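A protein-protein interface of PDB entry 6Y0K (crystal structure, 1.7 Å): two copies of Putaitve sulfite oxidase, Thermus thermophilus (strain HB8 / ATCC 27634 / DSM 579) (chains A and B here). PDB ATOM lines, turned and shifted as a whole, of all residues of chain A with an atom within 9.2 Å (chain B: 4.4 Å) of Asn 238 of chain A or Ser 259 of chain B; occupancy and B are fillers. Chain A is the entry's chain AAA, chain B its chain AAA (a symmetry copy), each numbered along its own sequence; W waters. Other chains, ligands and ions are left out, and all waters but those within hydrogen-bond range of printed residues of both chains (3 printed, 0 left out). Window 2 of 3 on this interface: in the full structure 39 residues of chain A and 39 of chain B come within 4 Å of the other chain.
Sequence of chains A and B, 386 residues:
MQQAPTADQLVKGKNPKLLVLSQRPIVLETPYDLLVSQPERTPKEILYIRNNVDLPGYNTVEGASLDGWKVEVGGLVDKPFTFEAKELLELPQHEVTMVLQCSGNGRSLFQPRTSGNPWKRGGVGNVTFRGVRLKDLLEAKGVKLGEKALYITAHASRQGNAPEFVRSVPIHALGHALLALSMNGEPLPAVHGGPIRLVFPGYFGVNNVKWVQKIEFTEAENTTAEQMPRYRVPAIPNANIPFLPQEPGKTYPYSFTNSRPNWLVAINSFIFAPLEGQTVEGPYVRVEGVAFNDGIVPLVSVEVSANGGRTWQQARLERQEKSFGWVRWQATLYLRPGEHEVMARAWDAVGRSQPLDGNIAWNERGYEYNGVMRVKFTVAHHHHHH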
ATOM      1  N   ALA A 235     -24.624  26.005  20.946  1.00  0.00           N
ATOM      2  CA  ALA A 235     -23.209  25.710  20.664  1.00  0.00           C
ATOM      3  C   ALA A 235     -23.085  24.427  19.863  1.00  0.00           C
ATOM      4  O   ALA A 235     -24.038  23.623  19.824  1.00  0.00           O
ATOM      5  CB  ALA A 235     -22.472  25.586  21.964  1.00  0.00           C
ATOM      6  N   ILE A 236     -21.912  24.241  19.270  1.00  0.00           N
ATOM      7  CA  ILE A 236     -21.465  22.917  18.776  1.00  0.00           C
ATOM      8  C   ILE A 236     -20.501  22.391  19.824  1.00  0.00           C
ATOM      9  O   ILE A 236     -19.432  22.968  19.989  1.00  0.00           O
ATOM     10  CB  ILE A 236     -20.788  23.022  17.406  1.00  0.00           C
ATOM     11  CG1 ILE A 236     -21.663  23.731  16.364  1.00  0.00           C
ATOM     12  CG2 ILE A 236     -20.367  21.625  16.978  1.00  0.00           C
ATOM     13  CD1 ILE A 236     -20.966  24.030  15.072  1.00  0.00           C
ATOM     14  N   PRO A 237     -20.894  21.394  20.642  1.00  0.00           N
ATOM     15  CA  PRO A 237     -20.063  20.994  21.772  1.00  0.00           C
ATOM     16  C   PRO A 237     -18.642  20.620  21.332  1.00  0.00           C
ATOM     17  O   PRO A 237     -18.477  19.880  20.372  1.00  0.00           O
ATOM     18  CB  PRO A 237     -20.827  19.821  22.392  1.00  0.00           C
ATOM     19  CG  PRO A 237     -22.278  20.173  22.055  1.00  0.00           C
ATOM     20  CD  PRO A 237     -22.204  20.714  20.644  1.00  0.00           C
ATOM     21  N   ASN A 238     -17.675  21.185  22.045  1.00  0.00           N
ATOM     22  CA  ASN A 238     -16.227  20.907  21.911  1.00  0.00           C
ATOM     23  C   ASN A 238     -15.722  21.348  20.533  1.00  0.00           C
ATOM     24  O   ASN A 238     -14.711  20.818  20.091  1.00  0.00           O
ATOM     25  CB  ASN A 238     -15.913  19.435  22.198  1.00  0.00           C
ATOM     26  CG  ASN A 238     -14.682  19.285  23.065  1.00  0.00           C
ATOM     27  OD1 ASN A 238     -14.176  20.270  23.636  1.00  0.00           O
ATOM     28  ND2 ASN A 238     -14.159  18.069  23.129  1.00  0.00           N
ATOM     29  N   ALA A 239     -16.400  22.293  19.874  1.00  0.00           N
ATOM     30  CA  ALA A 239     -15.957  22.900  18.606  1.00  0.00           C
ATOM     31  C   ALA A 239     -15.554  24.349  18.896  1.00  0.00           C
ATOM     32  O   ALA A 239     -16.149  24.981  19.783  1.00  0.00           O
ATOM     33  CB  ALA A 239     -17.030  22.799  17.553  1.00  0.00           C
ATOM     34  N   ASN A 240     -14.605  24.864  18.131  1.00  0.00           N
ATOM     35  CA  ASN A 240     -14.018  26.201  18.360  1.00  0.00           C
ATOM     36  C   ASN A 240     -14.869  27.299  17.706  1.00  0.00           C
ATOM     37  O   ASN A 240     -14.448  27.880  16.689  1.00  0.00           O
ATOM     38  CB  ASN A 240     -12.575  26.238  17.871  1.00  0.00           C
ATOM     39  CG  ASN A 240     -11.928  27.577  18.153  1.00  0.00           C
ATOM     40  OD1 ASN A 240     -12.398  28.324  19.009  1.00  0.00           O
ATOM     41  ND2 ASN A 240     -10.885  27.912  17.407  1.00  0.00           N
ATOM     42  N   ILE A 241     -16.022  27.579  18.300  1.00  0.00           N
ATOM     43  CA  ILE A 241     -16.861  28.770  18.002  1.00  0.00           C
ATOM     44  C   ILE A 241     -17.520  29.158  19.316  1.00  0.00           C
ATOM     45  O   ILE A 241     -17.965  28.296  20.069  1.00  0.00           O
ATOM     46  CB  ILE A 241     -17.856  28.511  16.841  1.00  0.00           C
ATOM     47  CG1 ILE A 241     -18.472  29.823  16.351  1.00  0.00           C
ATOM     48  CG2 ILE A 241     -18.902  27.451  17.188  1.00  0.00           C
ATOM     49  CD1 ILE A 241     -19.314  29.711  15.101  1.00  0.00           C
ATOM     50  N   PHE A 256     -28.424  19.096  26.591  1.00  0.00           N
ATOM     51  CA  PHE A 256     -26.985  18.986  26.940  1.00  0.00           C
ATOM     52  C   PHE A 256     -26.122  18.916  25.684  1.00  0.00           C
ATOM     53  O   PHE A 256     -24.908  19.199  25.800  1.00  0.00           O
ATOM     54  CB  PHE A 256     -26.732  17.785  27.842  1.00  0.00           C
ATOM     55  CG  PHE A 256     -27.126  18.025  29.275  1.00  0.00           C
ATOM     56  CD1 PHE A 256     -26.439  18.947  30.052  1.00  0.00           C
ATOM     57  CD2 PHE A 256     -28.194  17.354  29.844  1.00  0.00           C
ATOM     58  CE1 PHE A 256     -26.787  19.162  31.377  1.00  0.00           C
ATOM     59  CE2 PHE A 256     -28.544  17.574  31.168  1.00  0.00           C
ATOM     60  CZ  PHE A 256     -27.844  18.480  31.933  1.00  0.00           C
ATOM     61  N   THR A 257     -26.663  18.489  24.543  1.00  0.00           N
ATOM     62  CA  THR A 257     -25.830  18.124  23.373  1.00  0.00           C
ATOM     63  C   THR A 257     -25.885  19.188  22.279  1.00  0.00           C
ATOM     64  O   THR A 257     -25.190  18.993  21.280  1.00  0.00           O
ATOM     65  CB  THR A 257     -26.207  16.726  22.856  1.00  0.00           C
ATOM     66  OG1 THR A 257     -27.554  16.714  22.401  1.00  0.00           O
ATOM     67  CG2 THR A 257     -26.025  15.678  23.926  1.00  0.00           C
ATOM     68  N   ASN A 258     -26.590  20.309  22.454  1.00  0.00           N
ATOM     69  CA  ASN A 258     -26.628  21.383  21.429  1.00  0.00           C
ATOM     70  C   ASN A 258     -26.471  22.769  22.068  1.00  0.00           C
ATOM     71  O   ASN A 258     -26.799  23.773  21.425  1.00  0.00           O
ATOM     72  CB  ASN A 258     -27.927  21.330  20.626  1.00  0.00           C
ATOM     73  CG  ASN A 258     -29.114  21.724  21.468  1.00  0.00           C
ATOM     74  OD1 ASN A 258     -28.969  22.134  22.616  1.00  0.00           O
ATOM     75  ND2 ASN A 258     -30.302  21.553  20.910  1.00  0.00           N
ATOM     76  N   SER A 259     -25.932  22.833  23.274  1.00  0.00           N
ATOM     77  CA  SER A 259     -25.802  24.111  24.008  1.00  0.00           C
ATOM     78  C   SER A 259     -24.730  23.957  25.075  1.00  0.00           C
ATOM     79  O   SER A 259     -24.434  22.825  25.478  1.00  0.00           O
ATOM     80  CB  SER A 259     -27.131  24.536  24.591  1.00  0.00           C
ATOM     81  OG  SER A 259     -27.543  23.669  25.628  1.00  0.00           O
ATOM     82  N   ARG A 260     -24.125  25.065  25.475  1.00  0.00           N
ATOM     83  CA  ARG A 260     -23.048  25.048  26.482  1.00  0.00           C
ATOM     84  C   ARG A 260     -23.476  25.934  27.638  1.00  0.00           C
ATOM     85  O   ARG A 260     -24.208  26.902  27.440  1.00  0.00           O
ATOM     86  CB  ARG A 260     -21.729  25.474  25.834  1.00  0.00           C
ATOM     87  CG  ARG A 260     -21.682  26.940  25.422  1.00  0.00           C
ATOM     88  CD  ARG A 260     -20.256  27.430  25.224  1.00  0.00           C
ATOM     89  NE  ARG A 260     -20.210  28.826  24.780  1.00  0.00           N
ATOM     90  CZ  ARG A 260     -20.460  29.888  25.559  1.00  0.00           C
ATOM     91  NH1 ARG A 260     -20.757  29.747  26.840  1.00  0.00           N
ATOM     92  NH2 ARG A 260     -20.416  31.104  25.056  1.00  0.00           N
ATOM     93  N   PRO A 261     -22.987  25.653  28.856  1.00  0.00           N
ATOM     94  CA  PRO A 261     -23.297  26.489  30.011  1.00  0.00           C
ATOM     95  C   PRO A 261     -22.623  27.863  29.941  1.00  0.00           C
ATOM     96  O   PRO A 261     -21.596  28.045  29.240  1.00  0.00           O
ATOM     97  CB  PRO A 261     -22.739  25.686  31.189  1.00  0.00           C
ATOM     98  CG  PRO A 261     -22.568  24.292  30.654  1.00  0.00           C
ATOM     99  CD  PRO A 261     -22.161  24.494  29.225  1.00  0.00           C
ATOM    100  N   TRP A 263     -20.157  29.667  31.484  1.00  0.00           N
ATOM    101  CA  TRP A 263     -18.963  29.322  32.271  1.00  0.00           C
ATOM    102  C   TRP A 263     -17.947  30.460  32.148  1.00  0.00           C
ATOM    103  O   TRP A 263     -18.055  31.419  32.928  1.00  0.00           O
ATOM    104  CB  TRP A 263     -18.411  27.960  31.833  1.00  0.00           C
ATOM    105  CG  TRP A 263     -19.091  26.775  32.447  1.00  0.00           C
ATOM    106  CD1 TRP A 263     -19.854  26.718  33.585  1.00  0.00           C
ATOM    107  CD2 TRP A 263     -18.996  25.429  31.961  1.00  0.00           C
ATOM    108  NE1 TRP A 263     -20.267  25.435  33.813  1.00  0.00           N
ATOM    109  CE2 TRP A 263     -19.752  24.621  32.838  1.00  0.00           C
ATOM    110  CE3 TRP A 263     -18.373  24.850  30.847  1.00  0.00           C
ATOM    111  CZ2 TRP A 263     -19.870  23.251  32.648  1.00  0.00           C
ATOM    112  CZ3 TRP A 263     -18.484  23.493  30.665  1.00  0.00           C
ATOM    113  CH2 TRP A 263     -19.238  22.714  31.554  1.00  0.00           C
ATOM    114  N   ARG B 232      -5.928  16.267  17.999  1.00  0.00           N
ATOM    115  CA  ARG B 232      -6.576  16.971  19.126  1.00  0.00           C
ATOM    116  C   ARG B 232      -5.646  18.036  19.697  1.00  0.00           C
ATOM    117  O   ARG B 232      -4.402  17.926  19.562  1.00  0.00           O
ATOM    118  CB  ARG B 232      -6.961  16.006  20.253  1.00  0.00           C
ATOM    119  CG  ARG B 232      -7.888  14.877  19.843  1.00  0.00           C
ATOM    120  CD  ARG B 232      -8.228  14.002  21.034  1.00  0.00           C
ATOM    121  NE  ARG B 232      -9.437  14.481  21.696  1.00  0.00           N
ATOM    122  CZ  ARG B 232     -10.682  14.211  21.308  1.00  0.00           C
ATOM    123  NH1 ARG B 232     -10.914  13.409  20.283  1.00  0.00           N
ATOM    124  NH2 ARG B 232     -11.700  14.738  21.966  1.00  0.00           N
ATOM    125  N   VAL B 233      -6.231  19.047  20.319  1.00  0.00           N
ATOM    126  CA  VAL B 233      -5.482  20.087  21.055  1.00  0.00           C
ATOM    127  C   VAL B 233      -6.075  20.193  22.444  1.00  0.00           C
ATOM    128  O   VAL B 233      -7.269  19.930  22.644  1.00  0.00           O
ATOM    129  CB  VAL B 233      -5.470  21.454  20.346  1.00  0.00           C
ATOM    130  CG1 VAL B 233      -4.837  21.341  18.975  1.00  0.00           C
ATOM    131  CG2 VAL B 233      -6.863  22.070  20.283  1.00  0.00           C
ATOM    132  N   PRO B 234      -5.266  20.586  23.446  1.00  0.00           N
ATOM    133  CA  PRO B 234      -5.778  20.752  24.811  1.00  0.00           C
ATOM    134  C   PRO B 234      -6.951  21.743  24.854  1.00  0.00           C
ATOM    135  O   PRO B 234      -6.914  22.744  24.165  1.00  0.00           O
ATOM    136  CB  PRO B 234      -4.564  21.279  25.588  1.00  0.00           C
ATOM    137  CG  PRO B 234      -3.384  20.749  24.786  1.00  0.00           C
ATOM    138  CD  PRO B 234      -3.825  20.899  23.345  1.00  0.00           C
ATOM    139  N   ALA B 235      -7.951  21.445  25.686  1.00  0.00           N
ATOM    140  CA  ALA B 235      -9.166  22.272  25.778  1.00  0.00           C
ATOM    141  C   ALA B 235      -9.851  22.060  27.115  1.00  0.00           C
ATOM    142  O   ALA B 235      -9.577  21.055  27.803  1.00  0.00           O
ATOM    143  CB  ALA B 235     -10.088  21.901  24.655  1.00  0.00           C
ATOM    144  N   PRO B 237     -13.515  21.172  27.742  1.00  0.00           N
ATOM    145  CA  PRO B 237     -14.637  20.794  26.891  1.00  0.00           C
ATOM    146  C   PRO B 237     -15.871  21.668  27.153  1.00  0.00           C
ATOM    147  O   PRO B 237     -16.233  21.883  28.301  1.00  0.00           O
ATOM    148  CB  PRO B 237     -14.868  19.317  27.223  1.00  0.00           C
ATOM    149  CG  PRO B 237     -13.460  18.852  27.600  1.00  0.00           C
ATOM    150  CD  PRO B 237     -12.898  20.004  28.403  1.00  0.00           C
ATOM    151  N   ASN B 238     -16.440  22.162  26.059  1.00  0.00           N
ATOM    152  CA  ASN B 238     -17.702  22.934  26.016  1.00  0.00           C
ATOM    153  C   ASN B 238     -17.542  24.265  26.758  1.00  0.00           C
ATOM    154  O   ASN B 238     -18.548  24.809  27.195  1.00  0.00           O
ATOM    155  CB  ASN B 238     -18.878  22.110  26.552  1.00  0.00           C
ATOM    156  CG  ASN B 238     -20.109  22.264  25.685  1.00  0.00           C
ATOM    157  OD1 ASN B 238     -20.042  22.806  24.566  1.00  0.00           O
ATOM    158  ND2 ASN B 238     -21.249  21.837  26.210  1.00  0.00           N
ATOM    159  N   TYR B 254      -3.319  13.505  26.645  1.00  0.00           N
ATOM    160  CA  TYR B 254      -4.569  13.648  25.852  1.00  0.00           C
ATOM    161  C   TYR B 254      -5.562  12.582  26.288  1.00  0.00           C
ATOM    162  O   TYR B 254      -5.207  11.381  26.339  1.00  0.00           O
ATOM    163  CB  TYR B 254      -4.317  13.522  24.348  1.00  0.00           C
ATOM    164  CG  TYR B 254      -3.668  14.742  23.769  1.00  0.00           C
ATOM    165  CD1 TYR B 254      -2.292  14.869  23.736  1.00  0.00           C
ATOM    166  CD2 TYR B 254      -4.429  15.791  23.287  1.00  0.00           C
ATOM    167  CE1 TYR B 254      -1.688  16.015  23.267  1.00  0.00           C
ATOM    168  CE2 TYR B 254      -3.845  16.946  22.814  1.00  0.00           C
ATOM    169  CZ  TYR B 254      -2.469  17.050  22.773  1.00  0.00           C
ATOM    170  OH  TYR B 254      -1.894  18.195  22.322  1.00  0.00           O
ATOM    171  N   SER B 255      -6.796  13.010  26.527  1.00  0.00           N
ATOM    172  CA  SER B 255      -7.964  12.125  26.681  1.00  0.00           C
ATOM    173  C   SER B 255      -9.165  12.756  25.974  1.00  0.00           C
ATOM    174  O   SER B 255      -9.075  13.931  25.563  1.00  0.00           O
ATOM    175  CB  SER B 255      -8.257  11.906  28.135  1.00  0.00           C
ATOM    176  OG  SER B 255      -8.858  13.067  28.684  1.00  0.00           O
ATOM    177  N   PHE B 256     -10.279  12.034  25.898  1.00  0.00           N
ATOM    178  CA  PHE B 256     -11.538  12.625  25.377  1.00  0.00           C
ATOM    179  C   PHE B 256     -11.984  13.805  26.234  1.00  0.00           C
ATOM    180  O   PHE B 256     -12.786  14.620  25.724  1.00  0.00           O
ATOM    181  CB  PHE B 256     -12.636  11.574  25.283  1.00  0.00           C
ATOM    182  CG  PHE B 256     -12.492  10.669  24.089  1.00  0.00           C
ATOM    183  CD1 PHE B 256     -12.646  11.166  22.802  1.00  0.00           C
ATOM    184  CD2 PHE B 256     -12.179   9.329  24.241  1.00  0.00           C
ATOM    185  CE1 PHE B 256     -12.529  10.334  21.699  1.00  0.00           C
ATOM    186  CE2 PHE B 256     -12.058   8.500  23.136  1.00  0.00           C
ATOM    187  CZ  PHE B 256     -12.228   9.003  21.866  1.00  0.00           C
ATOM    188  N   THR B 257     -11.573  13.884  27.500  1.00  0.00           N
ATOM    189  CA  THR B 257     -12.189  14.827  28.462  1.00  0.00           C
ATOM    190  C   THR B 257     -11.284  16.026  28.745  1.00  0.00           C
ATOM    191  O   THR B 257     -11.728  16.889  29.503  1.00  0.00           O
ATOM    192  CB  THR B 257     -12.613  14.094  29.745  1.00  0.00           C
ATOM    193  OG1 THR B 257     -11.476  13.547  30.400  1.00  0.00           O
ATOM    194  CG2 THR B 257     -13.601  12.993  29.445  1.00  0.00           C
ATOM    195  N   ASN B 258     -10.110  16.153  28.121  1.00  0.00           N
ATOM    196  CA  ASN B 258      -9.228  17.330  28.339  1.00  0.00           C
ATOM    197  C   ASN B 258      -8.666  17.857  27.013  1.00  0.00           C
ATOM    198  O   ASN B 258      -7.681  18.605  27.028  1.00  0.00           O
ATOM    199  CB  ASN B 258      -8.079  16.984  29.284  1.00  0.00           C
ATOM    200  CG  ASN B 258      -7.100  16.032  28.643  1.00  0.00           C
ATOM    201  OD1 ASN B 258      -7.215  15.706  27.464  1.00  0.00           O
ATOM    202  ND2 ASN B 258      -6.159  15.546  29.436  1.00  0.00           N
ATOM    203  N   SER B 259      -9.304  17.532  25.900  1.00  0.00           N
ATOM    204  CA  SER B 259      -8.804  17.929  24.566  1.00  0.00           C
ATOM    205  C   SER B 259      -9.956  17.871  23.574  1.00  0.00           C
ATOM    206  O   SER B 259     -10.941  17.167  23.831  1.00  0.00           O
ATOM    207  CB  SER B 259      -7.643  17.057  24.142  1.00  0.00           C
ATOM    208  OG  SER B 259      -8.056  15.728  23.894  1.00  0.00           O
ATOM    209  N   ARG B 260      -9.856  18.640  22.501  1.00  0.00           N
ATOM    210  CA  ARG B 260     -10.918  18.697  21.479  1.00  0.00           C
ATOM    211  C   ARG B 260     -10.306  18.300  20.148  1.00  0.00           C
ATOM    212  O   ARG B 260      -9.122  18.536  19.914  1.00  0.00           O
ATOM    213  CB  ARG B 260     -11.554  20.089  21.475  1.00  0.00           C
ATOM    214  CG  ARG B 260     -10.636  21.192  20.965  1.00  0.00           C
ATOM    215  CD  ARG B 260     -11.414  22.430  20.543  1.00  0.00           C
ATOM    216  NE  ARG B 260     -10.529  23.510  20.098  1.00  0.00           N
ATOM    217  CZ  ARG B 260      -9.872  23.532  18.931  1.00  0.00           C
ATOM    218  NH1 ARG B 260      -9.997  22.552  18.051  1.00  0.00           N
ATOM    219  NH2 ARG B 260      -9.081  24.542  18.634  1.00  0.00           N
ATOM    220  N   PRO B 261     -11.112  17.740  19.233  1.00  0.00           N
ATOM    221  CA  PRO B 261     -10.620  17.384  17.905  1.00  0.00           C
ATOM    222  C   PRO B 261     -10.318  18.611  17.040  1.00  0.00           C
ATOM    223  O   PRO B 261     -10.860  19.720  17.279  1.00  0.00           O
ATOM    224  CB  PRO B 261     -11.779  16.586  17.301  1.00  0.00           C
ATOM    225  CG  PRO B 261     -12.624  16.188  18.480  1.00  0.00           C
ATOM    226  CD  PRO B 261     -12.517  17.353  19.418  1.00  0.00           C
ATOM    227  N   TRP B 263     -11.497  20.236  14.268  1.00  0.00           N
ATOM    228  CA  TRP B 263     -12.796  20.298  13.582  1.00  0.00           C
ATOM    229  C   TRP B 263     -12.888  21.624  12.820  1.00  0.00           C
ATOM    230  O   TRP B 263     -12.402  21.671  11.680  1.00  0.00           O
ATOM    231  CB  TRP B 263     -13.939  20.090  14.584  1.00  0.00           C
ATOM    232  CG  TRP B 263     -14.241  18.659  14.909  1.00  0.00           C
ATOM    233  CD1 TRP B 263     -13.922  17.532  14.196  1.00  0.00           C
ATOM    234  CD2 TRP B 263     -15.007  18.216  16.037  1.00  0.00           C
ATOM    235  NE1 TRP B 263     -14.408  16.420  14.826  1.00  0.00           N
ATOM    236  CE2 TRP B 263     -15.083  16.808  15.955  1.00  0.00           C
ATOM    237  CE3 TRP B 263     -15.598  18.881  17.120  1.00  0.00           C
ATOM    238  CZ2 TRP B 263     -15.762  16.058  16.905  1.00  0.00           C
ATOM    239  CZ3 TRP B 263     -16.275  18.138  18.055  1.00  0.00           C
ATOM    240  CH2 TRP B 263     -16.338  16.742  17.947  1.00  0.00           C
HETATM  241  O   HOH W   1     -13.039  20.933  17.963  1.00  0.00           O
HETATM  242  O   HOH W   2     -19.329  27.067  28.472  1.00  0.00           O
HETATM  243  O   HOH W   3     -16.227  23.884  23.259  1.00  0.00           O
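ND2 of Asn 238 of chain A lies within hydrogen-bond range of O of Ser 259 of chain B (3.4 Å).
ND2 of Asn 238 of chain B is in hydrogen-bond range of O of Ser 259 of chain A (3.4 Å).
OG of Ser 259 of chain B lies within hydrogen-bond range of O of Ser 255 of chain B (2.7 Å).
NE of Arg 232 of chain B is in hydrogen-bond range of OG of Ser 259 of chain B (2.9 Å).
The backbone carbonyl oxygen (O) of Val 233 of chain B lies within hydrogen-bond range of the backbone NH (N) of Arg 260 of chain B (2.9 Å).
Pro 237 of chain A touches Asn 238 of chain B (CA to OD1, 3.3 Å).
O of Pro 237 of chain A touches CZ3 of Trp 263 of chain B, at 3.6 Å.
OD1 of Asn 238 of chain A touches CA of Pro 237 of chain B (3.3 Å).
Asn 238 of chain A touches Asn 238 of chain B.
Asn 238 of chain A touches Arg 260 of chain B (OD1 to CB, 3.4 Å).
Asn 238 of chain A touches Trp 263 of chain B (O to CE3, 3.7 Å).
Asn 240 of chain A touches Arg 260 of chain B.
Arg 260 of chain A touches Asn 238 of chain B.
Trp 263 of chain A touches Pro 237 of chain B.
CE3 of Trp 263 of chain A touches O of Asn 238 of chain B, 3.7 Å away.
Ala 235 of chain A touches none of the printed residues of chain B.
Printed residues of chain B within 4 Å of Pro 237 of chain A: Asn 238 and Trp 263.
Of chain B, only Pro 237, Asn 238, Ser 259, Arg 260 and Trp 263 come within 4 Å of Asn 238 of chain A.
Printed residues of chain B within 4 Å of Asn 240 of chain A: Arg 260 (3.96 Å).
Printed residues of chain B within 4 Å of Ser 259 of chain A: Asn 238 (3.4 Å).
No residue of chain A comes within 4 Å of Ala 235 of chain B.
Printed residues of chain A within 4 Å of Pro 237 of chain B: Asn 238 and Trp 263.
Of the printed residues of chain A, Asn 238 of chain B touches Pro 237, Asn 238, Ser 259, Arg 260 and Trp 263.
Tyr 254 of chain B touches none of the printed residues of chain A.
Ser 259 of chain B touches just one residue of chain A: Asn 238.
The nearest printed residue of chain A that does not touch Asn 238 of chain B is Pro 261 of chain A (4.1 Å).
Hydrophobic or aromatic side chains of chain B within 4 Å of the printed part of chain A: Pro 237 and Trp 263.
Printed residues of chain A that touch a printed residue of chain B: Pro 237, Asn 238, Asn 240, Ser 259, Arg 260 and Trp 263.
Hydrophobic or aromatic side chains of chain A that line the printed part of chain B: Pro 237 and Trp 263.
Among the printed residues, no Asp or Glu carboxylate lies within 4 Å of a Lys or Arg side-chain nitrogen of the other chain.
Pro 237 of chain A touches Asn 238 of chain B, and with the chains exchanged Asn 238 of chain A touches Pro 237 of chain B.
Asn 238 of chain B touches its own counterpart, Asn 238 of chain A.
Asn 238 of chain A touches Ser 259 of chain B, and with the chains exchanged Ser 259 of chain A touches Asn 238 of chain B.
Asn 238 of chain A touches Arg 260 of chain B, and with the chains exchanged Arg 260 of chain A touches Asn 238 of chain B.
Positions printed for both chains: 235, 237, 238, 256, 257, 258, 259, 260, 261 and 263.
Of the 12 pairs that touch across the chains among the printed residues, 11 have their exchanged pair printed and touching as well.
Water W2 lies within hydrogen-bond range of O of Pro 261 of chain A, O of Asn 238 of chain B and NH1 of Arg 260 of chain A.
Water W1 lies within hydrogen-bond range of the backbone carbonyl oxygen of Pro 261 of chain B, the backbone carbonyl oxygen of Asn 238 of chain A and the guanidinium group of Arg 260 of chain B.
Water W3 lies within hydrogen-bond range of N of Asn 238 of chain B (3.3 Å) and N of Asn 238 of chain A (3.3 Å).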
